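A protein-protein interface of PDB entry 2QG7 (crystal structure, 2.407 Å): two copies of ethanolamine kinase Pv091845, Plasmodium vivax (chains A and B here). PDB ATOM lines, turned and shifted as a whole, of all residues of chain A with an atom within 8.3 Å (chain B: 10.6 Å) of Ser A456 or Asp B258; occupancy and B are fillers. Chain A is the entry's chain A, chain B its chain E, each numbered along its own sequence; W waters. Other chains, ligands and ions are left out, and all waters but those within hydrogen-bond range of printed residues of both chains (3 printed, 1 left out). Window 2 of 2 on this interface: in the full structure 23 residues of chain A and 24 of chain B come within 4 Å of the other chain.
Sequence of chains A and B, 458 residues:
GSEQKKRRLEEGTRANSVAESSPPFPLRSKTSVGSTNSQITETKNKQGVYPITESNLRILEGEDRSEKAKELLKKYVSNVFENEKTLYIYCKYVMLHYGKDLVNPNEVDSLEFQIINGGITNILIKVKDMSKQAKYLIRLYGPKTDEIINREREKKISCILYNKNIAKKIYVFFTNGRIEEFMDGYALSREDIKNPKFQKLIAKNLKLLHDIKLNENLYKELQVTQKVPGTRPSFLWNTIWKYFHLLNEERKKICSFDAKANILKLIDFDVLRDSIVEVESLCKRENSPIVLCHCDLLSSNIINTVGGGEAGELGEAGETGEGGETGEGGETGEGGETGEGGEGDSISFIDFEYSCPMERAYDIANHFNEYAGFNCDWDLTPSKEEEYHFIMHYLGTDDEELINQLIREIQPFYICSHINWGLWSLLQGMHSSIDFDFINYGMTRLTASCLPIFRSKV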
ATOM      1  N   GLU A 278      -8.171 -16.548 -13.299  1.00  0.00           N
ATOM      2  CA  GLU A 278      -8.339 -15.116 -13.464  1.00  0.00           C
ATOM      3  C   GLU A 278      -9.797 -14.698 -13.356  1.00  0.00           C
ATOM      4  O   GLU A 278     -10.082 -13.707 -12.701  1.00  0.00           O
ATOM      5  CB  GLU A 278      -7.701 -14.657 -14.764  1.00  0.00           C
ATOM      6  CG  GLU A 278      -7.582 -13.144 -14.902  1.00  0.00           C
ATOM      7  CD  GLU A 278      -6.714 -12.682 -16.104  1.00  0.00           C
ATOM      8  OE1 GLU A 278      -6.787 -13.322 -17.192  1.00  0.00           O
ATOM      9  OE2 GLU A 278      -5.979 -11.657 -15.957  1.00  0.00           O
ATOM     10  N   GLN A 411     -21.032  -8.232 -14.156  1.00  0.00           N
ATOM     11  CA  GLN A 411     -20.128  -8.187 -15.348  1.00  0.00           C
ATOM     12  C   GLN A 411     -19.143  -9.340 -15.624  1.00  0.00           C
ATOM     13  O   GLN A 411     -19.139  -9.847 -16.752  1.00  0.00           O
ATOM     14  CB  GLN A 411     -19.353  -6.870 -15.438  1.00  0.00           C
ATOM     15  CG  GLN A 411     -20.260  -5.662 -15.559  1.00  0.00           C
ATOM     16  CD  GLN A 411     -21.184  -5.720 -16.756  1.00  0.00           C
ATOM     17  OE1 GLN A 411     -20.722  -5.693 -17.876  1.00  0.00           O
ATOM     18  NE2 GLN A 411     -22.495  -5.734 -16.521  1.00  0.00           N
ATOM     19  N   ILE A 415     -18.307 -14.155 -18.657  1.00  0.00           N
ATOM     20  CA  ILE A 415     -17.210 -15.041 -18.997  1.00  0.00           C
ATOM     21  C   ILE A 415     -17.253 -16.363 -18.231  1.00  0.00           C
ATOM     22  O   ILE A 415     -17.022 -17.431 -18.790  1.00  0.00           O
ATOM     23  CB  ILE A 415     -15.829 -14.380 -18.754  1.00  0.00           C
ATOM     24  CG1 ILE A 415     -15.690 -13.059 -19.523  1.00  0.00           C
ATOM     25  CG2 ILE A 415     -14.724 -15.283 -19.234  1.00  0.00           C
ATOM     26  CD1 ILE A 415     -14.543 -12.132 -18.929  1.00  0.00           C
ATOM     27  N   ALA A 448     -16.272 -17.569 -26.859  1.00  0.00           N
ATOM     28  CA  ALA A 448     -16.949 -16.405 -26.323  1.00  0.00           C
ATOM     29  C   ALA A 448     -16.282 -15.852 -25.045  1.00  0.00           C
ATOM     30  O   ALA A 448     -16.234 -14.632 -24.801  1.00  0.00           O
ATOM     31  CB  ALA A 448     -18.396 -16.741 -26.058  1.00  0.00           C
ATOM     32  N   SER A 449     -15.785 -16.765 -24.223  1.00  0.00           N
ATOM     33  CA  SER A 449     -14.988 -16.414 -23.042  1.00  0.00           C
ATOM     34  C   SER A 449     -13.698 -15.594 -23.364  1.00  0.00           C
ATOM     35  O   SER A 449     -13.170 -14.899 -22.511  1.00  0.00           O
ATOM     36  CB  SER A 449     -14.709 -17.654 -22.194  1.00  0.00           C
ATOM     37  OG  SER A 449     -13.695 -18.425 -22.782  1.00  0.00           O
ATOM     38  N   CYS A 450     -13.249 -15.636 -24.605  1.00  0.00           N
ATOM     39  CA  CYS A 450     -12.020 -14.948 -25.031  1.00  0.00           C
ATOM     40  C   CYS A 450     -12.309 -13.732 -25.893  1.00  0.00           C
ATOM     41  O   CYS A 450     -11.377 -13.025 -26.266  1.00  0.00           O
ATOM     42  CB  CYS A 450     -11.143 -15.869 -25.849  1.00  0.00           C
ATOM     43  SG  CYS A 450     -10.552 -17.322 -24.983  1.00  0.00           S
ATOM     44  N   LEU A 451     -13.590 -13.505 -26.200  1.00  0.00           N
ATOM     45  CA  LEU A 451     -13.991 -12.461 -27.145  1.00  0.00           C
ATOM     46  C   LEU A 451     -13.988 -11.130 -26.448  1.00  0.00           C
ATOM     47  O   LEU A 451     -14.490 -11.051 -25.340  1.00  0.00           O
ATOM     48  CB  LEU A 451     -15.396 -12.728 -27.705  1.00  0.00           C
ATOM     49  CG  LEU A 451     -15.530 -13.764 -28.835  1.00  0.00           C
ATOM     50  CD1 LEU A 451     -16.970 -13.844 -29.300  1.00  0.00           C
ATOM     51  CD2 LEU A 451     -14.662 -13.400 -30.001  1.00  0.00           C
ATOM     52  N   PRO A 452     -13.469 -10.074 -27.090  1.00  0.00           N
ATOM     53  CA  PRO A 452     -13.486  -8.745 -26.482  1.00  0.00           C
ATOM     54  C   PRO A 452     -14.859  -8.270 -25.989  1.00  0.00           C
ATOM     55  O   PRO A 452     -14.932  -7.527 -24.980  1.00  0.00           O
ATOM     56  CB  PRO A 452     -13.047  -7.834 -27.633  1.00  0.00           C
ATOM     57  CG  PRO A 452     -12.210  -8.712 -28.520  1.00  0.00           C
ATOM     58  CD  PRO A 452     -12.844 -10.064 -28.429  1.00  0.00           C
ATOM     59  N   ILE A 453     -15.936  -8.617 -26.706  1.00  0.00           N
ATOM     60  CA  ILE A 453     -17.259  -8.123 -26.322  1.00  0.00           C
ATOM     61  C   ILE A 453     -17.660  -8.615 -24.933  1.00  0.00           C
ATOM     62  O   ILE A 453     -18.501  -8.012 -24.289  1.00  0.00           O
ATOM     63  CB  ILE A 453     -18.356  -8.495 -27.333  1.00  0.00           C
ATOM     64  CG1 ILE A 453     -18.275  -9.977 -27.670  1.00  0.00           C
ATOM     65  CG2 ILE A 453     -18.193  -7.655 -28.589  1.00  0.00           C
ATOM     66  CD1 ILE A 453     -19.533 -10.534 -28.369  1.00  0.00           C
ATOM     67  N   PHE A 454     -17.092  -9.730 -24.495  1.00  0.00           N
ATOM     68  CA  PHE A 454     -17.355 -10.196 -23.146  1.00  0.00           C
ATOM     69  C   PHE A 454     -16.244  -9.776 -22.165  1.00  0.00           C
ATOM     70  O   PHE A 454     -16.544  -9.468 -21.002  1.00  0.00           O
ATOM     71  CB  PHE A 454     -17.655 -11.696 -23.104  1.00  0.00           C
ATOM     72  CG  PHE A 454     -18.951 -12.051 -23.743  1.00  0.00           C
ATOM     73  CD1 PHE A 454     -18.986 -12.679 -25.015  1.00  0.00           C
ATOM     74  CD2 PHE A 454     -20.147 -11.686 -23.140  1.00  0.00           C
ATOM     75  CE1 PHE A 454     -20.151 -12.993 -25.630  1.00  0.00           C
ATOM     76  CE2 PHE A 454     -21.373 -11.983 -23.763  1.00  0.00           C
ATOM     77  CZ  PHE A 454     -21.352 -12.680 -25.036  1.00  0.00           C
ATOM     78  N   ARG A 455     -14.988  -9.774 -22.621  1.00  0.00           N
ATOM     79  CA  ARG A 455     -13.833  -9.466 -21.778  1.00  0.00           C
ATOM     80  C   ARG A 455     -13.752  -7.991 -21.398  1.00  0.00           C
ATOM     81  O   ARG A 455     -13.139  -7.631 -20.368  1.00  0.00           O
ATOM     82  CB  ARG A 455     -12.511  -9.849 -22.461  1.00  0.00           C
ATOM     83  CG  ARG A 455     -12.367 -11.301 -22.759  1.00  0.00           C
ATOM     84  CD  ARG A 455     -11.887 -12.134 -21.560  1.00  0.00           C
ATOM     85  NE  ARG A 455     -10.452 -12.328 -21.663  1.00  0.00           N
ATOM     86  CZ  ARG A 455      -9.836 -13.502 -21.717  1.00  0.00           C
ATOM     87  NH1 ARG A 455      -8.525 -13.525 -21.783  1.00  0.00           N
ATOM     88  NH2 ARG A 455     -10.503 -14.644 -21.691  1.00  0.00           N
ATOM     89  N   SER A 456     -14.347  -7.143 -22.238  1.00  0.00           N
ATOM     90  CA  SER A 456     -14.277  -5.702 -22.061  1.00  0.00           C
ATOM     91  C   SER A 456     -15.317  -5.201 -21.074  1.00  0.00           C
ATOM     92  O   SER A 456     -15.308  -4.040 -20.694  1.00  0.00           O
ATOM     93  CB  SER A 456     -14.379  -4.987 -23.408  1.00  0.00           C
ATOM     94  OG  SER A 456     -15.688  -5.091 -23.903  1.00  0.00           O
ATOM     95  N   LYS A 457     -16.216  -6.088 -20.670  1.00  0.00           N
ATOM     96  CA  LYS A 457     -17.270  -5.781 -19.722  1.00  0.00           C
ATOM     97  C   LYS A 457     -16.687  -5.663 -18.293  1.00  0.00           C
ATOM     98  O   LYS A 457     -17.223  -4.964 -17.446  1.00  0.00           O
ATOM     99  CB  LYS A 457     -18.298  -6.913 -19.714  1.00  0.00           C
ATOM    100  CG  LYS A 457     -19.254  -6.940 -20.816  1.00  0.00           C
ATOM    101  CD  LYS A 457     -20.134  -8.178 -20.662  1.00  0.00           C
ATOM    102  CE  LYS A 457     -20.953  -8.431 -21.931  1.00  0.00           C
ATOM    103  NZ  LYS A 457     -21.939  -7.287 -22.174  1.00  0.00           N
ATOM    104  N   VAL A 458     -15.618  -6.407 -18.044  1.00  0.00           N
ATOM    105  CA  VAL A 458     -15.000  -6.515 -16.743  1.00  0.00           C
ATOM    106  C   VAL A 458     -14.245  -5.235 -16.315  1.00  0.00           C
ATOM    107  O   VAL A 458     -13.915  -4.391 -17.177  1.00  0.00           O
ATOM    108  CB  VAL A 458     -14.022  -7.729 -16.706  1.00  0.00           C
ATOM    109  CG1 VAL A 458     -13.214  -7.688 -15.388  1.00  0.00           C
ATOM    110  CG2 VAL A 458     -14.823  -9.056 -16.808  1.00  0.00           C
ATOM    111  N   ILE B 254       2.321 -10.508 -25.330  1.00  0.00           N
ATOM    112  CA  ILE B 254       1.455 -10.348 -24.172  1.00  0.00           C
ATOM    113  C   ILE B 254       0.543  -9.163 -24.476  1.00  0.00           C
ATOM    114  O   ILE B 254       1.002  -8.094 -24.860  1.00  0.00           O
ATOM    115  CB  ILE B 254       2.241 -10.229 -22.808  1.00  0.00           C
ATOM    116  CG1 ILE B 254       1.290  -9.835 -21.655  1.00  0.00           C
ATOM    117  CG2 ILE B 254       3.411  -9.253 -22.925  1.00  0.00           C
ATOM    118  CD1 ILE B 254       1.769 -10.326 -20.271  1.00  0.00           C
ATOM    119  N   CYS B 255      -0.758  -9.388 -24.329  1.00  0.00           N
ATOM    120  CA  CYS B 255      -1.752  -8.393 -24.675  1.00  0.00           C
ATOM    121  C   CYS B 255      -2.666  -8.124 -23.476  1.00  0.00           C
ATOM    122  O   CYS B 255      -2.558  -8.772 -22.430  1.00  0.00           O
ATOM    123  CB  CYS B 255      -2.569  -8.903 -25.879  1.00  0.00           C
ATOM    124  SG  CYS B 255      -3.293 -10.541 -25.612  1.00  0.00           S
ATOM    125  N   SER B 256      -3.561  -7.152 -23.640  1.00  0.00           N
ATOM    126  CA  SER B 256      -4.559  -6.831 -22.639  1.00  0.00           C
ATOM    127  C   SER B 256      -5.623  -7.925 -22.457  1.00  0.00           C
ATOM    128  O   SER B 256      -5.805  -8.803 -23.301  1.00  0.00           O
ATOM    129  CB  SER B 256      -5.201  -5.484 -22.969  1.00  0.00           C
ATOM    130  OG  SER B 256      -5.959  -5.530 -24.168  1.00  0.00           O
ATOM    131  N   PHE B 257      -6.323  -7.868 -21.335  1.00  0.00           N
ATOM    132  CA  PHE B 257      -7.349  -8.827 -21.014  1.00  0.00           C
ATOM    133  C   PHE B 257      -8.459  -8.878 -22.080  1.00  0.00           C
ATOM    134  O   PHE B 257      -9.138  -9.885 -22.220  1.00  0.00           O
ATOM    135  CB  PHE B 257      -7.949  -8.459 -19.634  1.00  0.00           C
ATOM    136  CG  PHE B 257      -8.942  -9.457 -19.095  1.00  0.00           C
ATOM    137  CD1 PHE B 257      -8.522 -10.691 -18.624  1.00  0.00           C
ATOM    138  CD2 PHE B 257     -10.294  -9.157 -19.064  1.00  0.00           C
ATOM    139  CE1 PHE B 257      -9.447 -11.614 -18.135  1.00  0.00           C
ATOM    140  CE2 PHE B 257     -11.221 -10.065 -18.567  1.00  0.00           C
ATOM    141  CZ  PHE B 257     -10.791 -11.295 -18.112  1.00  0.00           C
ATOM    142  N   ASP B 258      -8.660  -7.805 -22.819  1.00  0.00           N
ATOM    143  CA  ASP B 258      -9.777  -7.779 -23.771  1.00  0.00           C
ATOM    144  C   ASP B 258      -9.356  -7.623 -25.242  1.00  0.00           C
ATOM    145  O   ASP B 258     -10.137  -7.151 -26.085  1.00  0.00           O
ATOM    146  CB  ASP B 258     -10.761  -6.681 -23.377  1.00  0.00           C
ATOM    147  CG  ASP B 258     -10.167  -5.289 -23.523  1.00  0.00           C
ATOM    148  OD1 ASP B 258      -8.937  -5.125 -23.312  1.00  0.00           O
ATOM    149  OD2 ASP B 258     -10.933  -4.361 -23.862  1.00  0.00           O
ATOM    150  N   ALA B 259      -8.128  -8.027 -25.544  1.00  0.00           N
ATOM    151  CA  ALA B 259      -7.582  -7.969 -26.898  1.00  0.00           C
ATOM    152  C   ALA B 259      -8.093  -9.098 -27.800  1.00  0.00           C
ATOM    153  O   ALA B 259      -8.445 -10.202 -27.339  1.00  0.00           O
ATOM    154  CB  ALA B 259      -6.065  -7.988 -26.845  1.00  0.00           C
ATOM    155  N   LYS B 260      -8.130  -8.796 -29.094  1.00  0.00           N
ATOM    156  CA  LYS B 260      -8.533  -9.765 -30.137  1.00  0.00           C
ATOM    157  C   LYS B 260      -7.711 -11.041 -30.174  1.00  0.00           C
ATOM    158  O   LYS B 260      -8.254 -12.096 -30.459  1.00  0.00           O
ATOM    159  CB  LYS B 260      -8.479  -9.123 -31.509  1.00  0.00           C
ATOM    160  CG  LYS B 260      -9.512  -8.059 -31.714  1.00  0.00           C
ATOM    161  CD  LYS B 260      -9.294  -7.492 -33.105  1.00  0.00           C
ATOM    162  CE  LYS B 260      -9.974  -6.158 -33.273  1.00  0.00           C
ATOM    163  NZ  LYS B 260      -9.143  -5.114 -32.592  1.00  0.00           N
ATOM    164  N   ALA B 261      -6.423 -10.947 -29.861  1.00  0.00           N
ATOM    165  CA  ALA B 261      -5.504 -12.087 -29.882  1.00  0.00           C
ATOM    166  C   ALA B 261      -5.640 -13.109 -28.747  1.00  0.00           C
ATOM    167  O   ALA B 261      -4.925 -14.107 -28.745  1.00  0.00           O
ATOM    168  CB  ALA B 261      -4.094 -11.580 -29.953  1.00  0.00           C
ATOM    169  N   ASN B 262      -6.554 -12.886 -27.791  1.00  0.00           N
ATOM    170  CA  ASN B 262      -6.738 -13.780 -26.645  1.00  0.00           C
ATOM    171  C   ASN B 262      -7.289 -15.156 -27.007  1.00  0.00           C
ATOM    172  O   ASN B 262      -7.092 -16.115 -26.260  1.00  0.00           O
ATOM    173  CB  ASN B 262      -7.627 -13.143 -25.566  1.00  0.00           C
ATOM    174  CG  ASN B 262      -6.886 -12.127 -24.715  1.00  0.00           C
ATOM    175  OD1 ASN B 262      -5.794 -12.368 -24.239  1.00  0.00           O
ATOM    176  ND2 ASN B 262      -7.496 -10.984 -24.521  1.00  0.00           N
ATOM    177  N   ILE B 263      -7.993 -15.237 -28.138  1.00  0.00           N
ATOM    178  CA  ILE B 263      -8.484 -16.515 -28.711  1.00  0.00           C
ATOM    179  C   ILE B 263      -7.337 -17.441 -29.141  1.00  0.00           C
ATOM    180  O   ILE B 263      -7.449 -18.669 -29.076  1.00  0.00           O
ATOM    181  CB  ILE B 263      -9.500 -16.267 -29.890  1.00  0.00           C
ATOM    182  CG1 ILE B 263     -10.205 -17.570 -30.297  1.00  0.00           C
ATOM    183  CG2 ILE B 263      -8.817 -15.550 -31.099  1.00  0.00           C
ATOM    184  CD1 ILE B 263     -10.795 -18.382 -29.083  1.00  0.00           C
ATOM    185  N   LYS B 265      -4.465 -17.806 -27.659  1.00  0.00           N
ATOM    186  CA  LYS B 265      -3.815 -18.343 -26.476  1.00  0.00           C
ATOM    187  C   LYS B 265      -4.511 -19.576 -25.971  1.00  0.00           C
ATOM    188  O   LYS B 265      -3.908 -20.443 -25.405  1.00  0.00           O
ATOM    189  CB  LYS B 265      -3.732 -17.262 -25.413  1.00  0.00           C
ATOM    190  CG  LYS B 265      -2.843 -16.096 -25.897  1.00  0.00           C
ATOM    191  CD  LYS B 265      -2.582 -15.042 -24.833  1.00  0.00           C
ATOM    192  CE  LYS B 265      -1.578 -13.984 -25.323  1.00  0.00           C
ATOM    193  NZ  LYS B 265      -1.305 -12.990 -24.189  1.00  0.00           N
ATOM    194  N   GLY B 429      -9.387 -11.936 -38.277  1.00  0.00           N
ATOM    195  CA  GLY B 429      -9.971 -11.475 -37.045  1.00  0.00           C
ATOM    196  C   GLY B 429      -9.045 -10.649 -36.156  1.00  0.00           C
ATOM    197  O   GLY B 429      -9.523  -9.953 -35.262  1.00  0.00           O
ATOM    198  N   MET B 430      -7.733 -10.730 -36.374  1.00  0.00           N
ATOM    199  CA  MET B 430      -6.768  -9.888 -35.651  1.00  0.00           C
ATOM    200  C   MET B 430      -6.796  -8.438 -36.136  1.00  0.00           C
ATOM    201  O   MET B 430      -6.593  -7.503 -35.341  1.00  0.00           O
ATOM    202  CB  MET B 430      -5.331 -10.423 -35.766  1.00  0.00           C
ATOM    203  CG  MET B 430      -5.121 -11.834 -35.251  1.00  0.00           C
ATOM    204  SD  MET B 430      -5.531 -12.196 -33.509  1.00  0.00           S
ATOM    205  CE  MET B 430      -7.224 -12.784 -33.589  1.00  0.00           C
ATOM    206  N   SER B 432      -9.379  -6.671 -37.907  1.00  0.00           N
ATOM    207  CA  SER B 432     -10.768  -6.813 -38.353  1.00  0.00           C
ATOM    208  C   SER B 432     -11.484  -5.511 -38.776  1.00  0.00           C
ATOM    209  O   SER B 432     -11.596  -4.526 -37.987  1.00  0.00           O
ATOM    210  CB  SER B 432     -11.602  -7.583 -37.318  1.00  0.00           C
ATOM    211  OG  SER B 432     -11.828  -6.764 -36.155  1.00  0.00           O
ATOM    212  N   ILE B 439     -13.486 -14.687 -36.046  1.00  0.00           N
ATOM    213  CA  ILE B 439     -12.988 -15.508 -34.922  1.00  0.00           C
ATOM    214  C   ILE B 439     -13.790 -16.798 -34.740  1.00  0.00           C
ATOM    215  O   ILE B 439     -13.216 -17.870 -34.600  1.00  0.00           O
ATOM    216  CB  ILE B 439     -13.029 -14.724 -33.584  1.00  0.00           C
ATOM    217  CG1 ILE B 439     -12.254 -13.396 -33.700  1.00  0.00           C
ATOM    218  CG2 ILE B 439     -12.598 -15.621 -32.398  1.00  0.00           C
ATOM    219  CD1 ILE B 439     -10.780 -13.521 -34.066  1.00  0.00           C
HETATM  220  O   HOH W   1      -9.973 -13.230 -28.481  1.00  0.00           O
HETATM  221  O   HOH W   2      -7.150 -16.519 -23.666  1.00  0.00           O
HETATM  222  O   HOH W   3      -6.082 -14.861 -21.891  1.00  0.00           O
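Of chain B, only Asp B258 (3.5 Å) comes within 4 Å of Ser A456. Asp B258 touches just these residues of chain A: Pro A452, Arg A455 and Ser A456. Ala B259 touches none of the printed residues of chain A. Printed residues of chain A within 4 Å of Ile B439: Leu A451. Of the printed residues of chain B, Leu A451 touches Ile B439 (3.9 Å). Of the printed residues of chain B, Cys A450 touches Asn B262 and Ile B263. Phe A454 touches none of the printed residues of chain B. Lys A457 touches none of the printed residues of chain B. The nearest residue of chain B that does not touch Ser A456 is Phe B257 (5.5 Å). The nearest residue of chain A that does not touch Asp B258 is Leu A451 (5.5 Å). The nearest printed residue of chain A that does not touch Asn B262 is Leu A451 (6.0 Å).
The guanidinium group (NH2) of Arg A455 lies within hydrogen-bond range of the backbone carbonyl oxygen (O) of Ser A449 (2.8 Å). The backbone carbonyl oxygen of Pro A452 is in hydrogen-bond range of the side-chain hydroxyl of Ser A456, at 2.8 Å. The side-chain amide oxygen of Asn B262 is in hydrogen-bond range of the side-chain sulfur of Cys B255. OG of Ser B256 lies within hydrogen-bond range of OD1 of Asp B258 (3.1 Å). The backbone carbonyl oxygen (O) of Phe B257 sits at hydrogen-bond distance from the side-chain amide nitrogen (ND2) of Asn B262. O of Ala B259 lies within hydrogen-bond range of ND2 of Asn B262 (3.1 Å).
Water W2 bridges the backbone carbonyl oxygen of Asn B262 and the side-chain sulfur of Cys A450. Water W1 lies within hydrogen-bond range of O of Cys A450 (2.6 Å), N of Ile B263 (2.8 Å) and O of Lys B260 (2.9 Å). Water W3 lies within hydrogen-bond range of NH1 of Arg A455 (2.8 Å) and OD1 of Asn B262 (3.4 Å).
NE of Arg A455 sits at hydrogen-bond distance from O of Phe B257, 2.8 Å away.
Of the 15 printed residues of chain B, 5 touch a printed residue of chain A. Among the printed residues, 10 pairs touch across the chains. Among the printed residues, no Asp or Glu carboxylate lies within 4 Å of a Lys or Arg side-chain nitrogen of the other chain.
No position is printed for both chains. Of the 10 pairs that touch across the chains among the printed residues, none has its exchanged pair printed and touching as well.
Glu A278 touches Phe B257 (OE1 to CE1, 3.3 Å). Ile A415 touches Phe B257 (CD1 to CE2, 3.9 Å). Cys A450 touches Asn B262 (O to CB, 3.8 Å). Ile B263 touches Cys A450 (N to CB, 3.9 Å). CG2 of Ile B439 touches CD2 of Leu A451, 3.9 Å away. Pro A452 touches Asp B258 (CB to O, 3.4 Å). CB of Arg A455 touches CA of Asp B258, 3.7 Å away. NH1 of Arg A455 touches CG of Asn B262, 3.6 Å away. OD2 of Asp B258 touches CB of Ser A456, at 3.5 Å.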
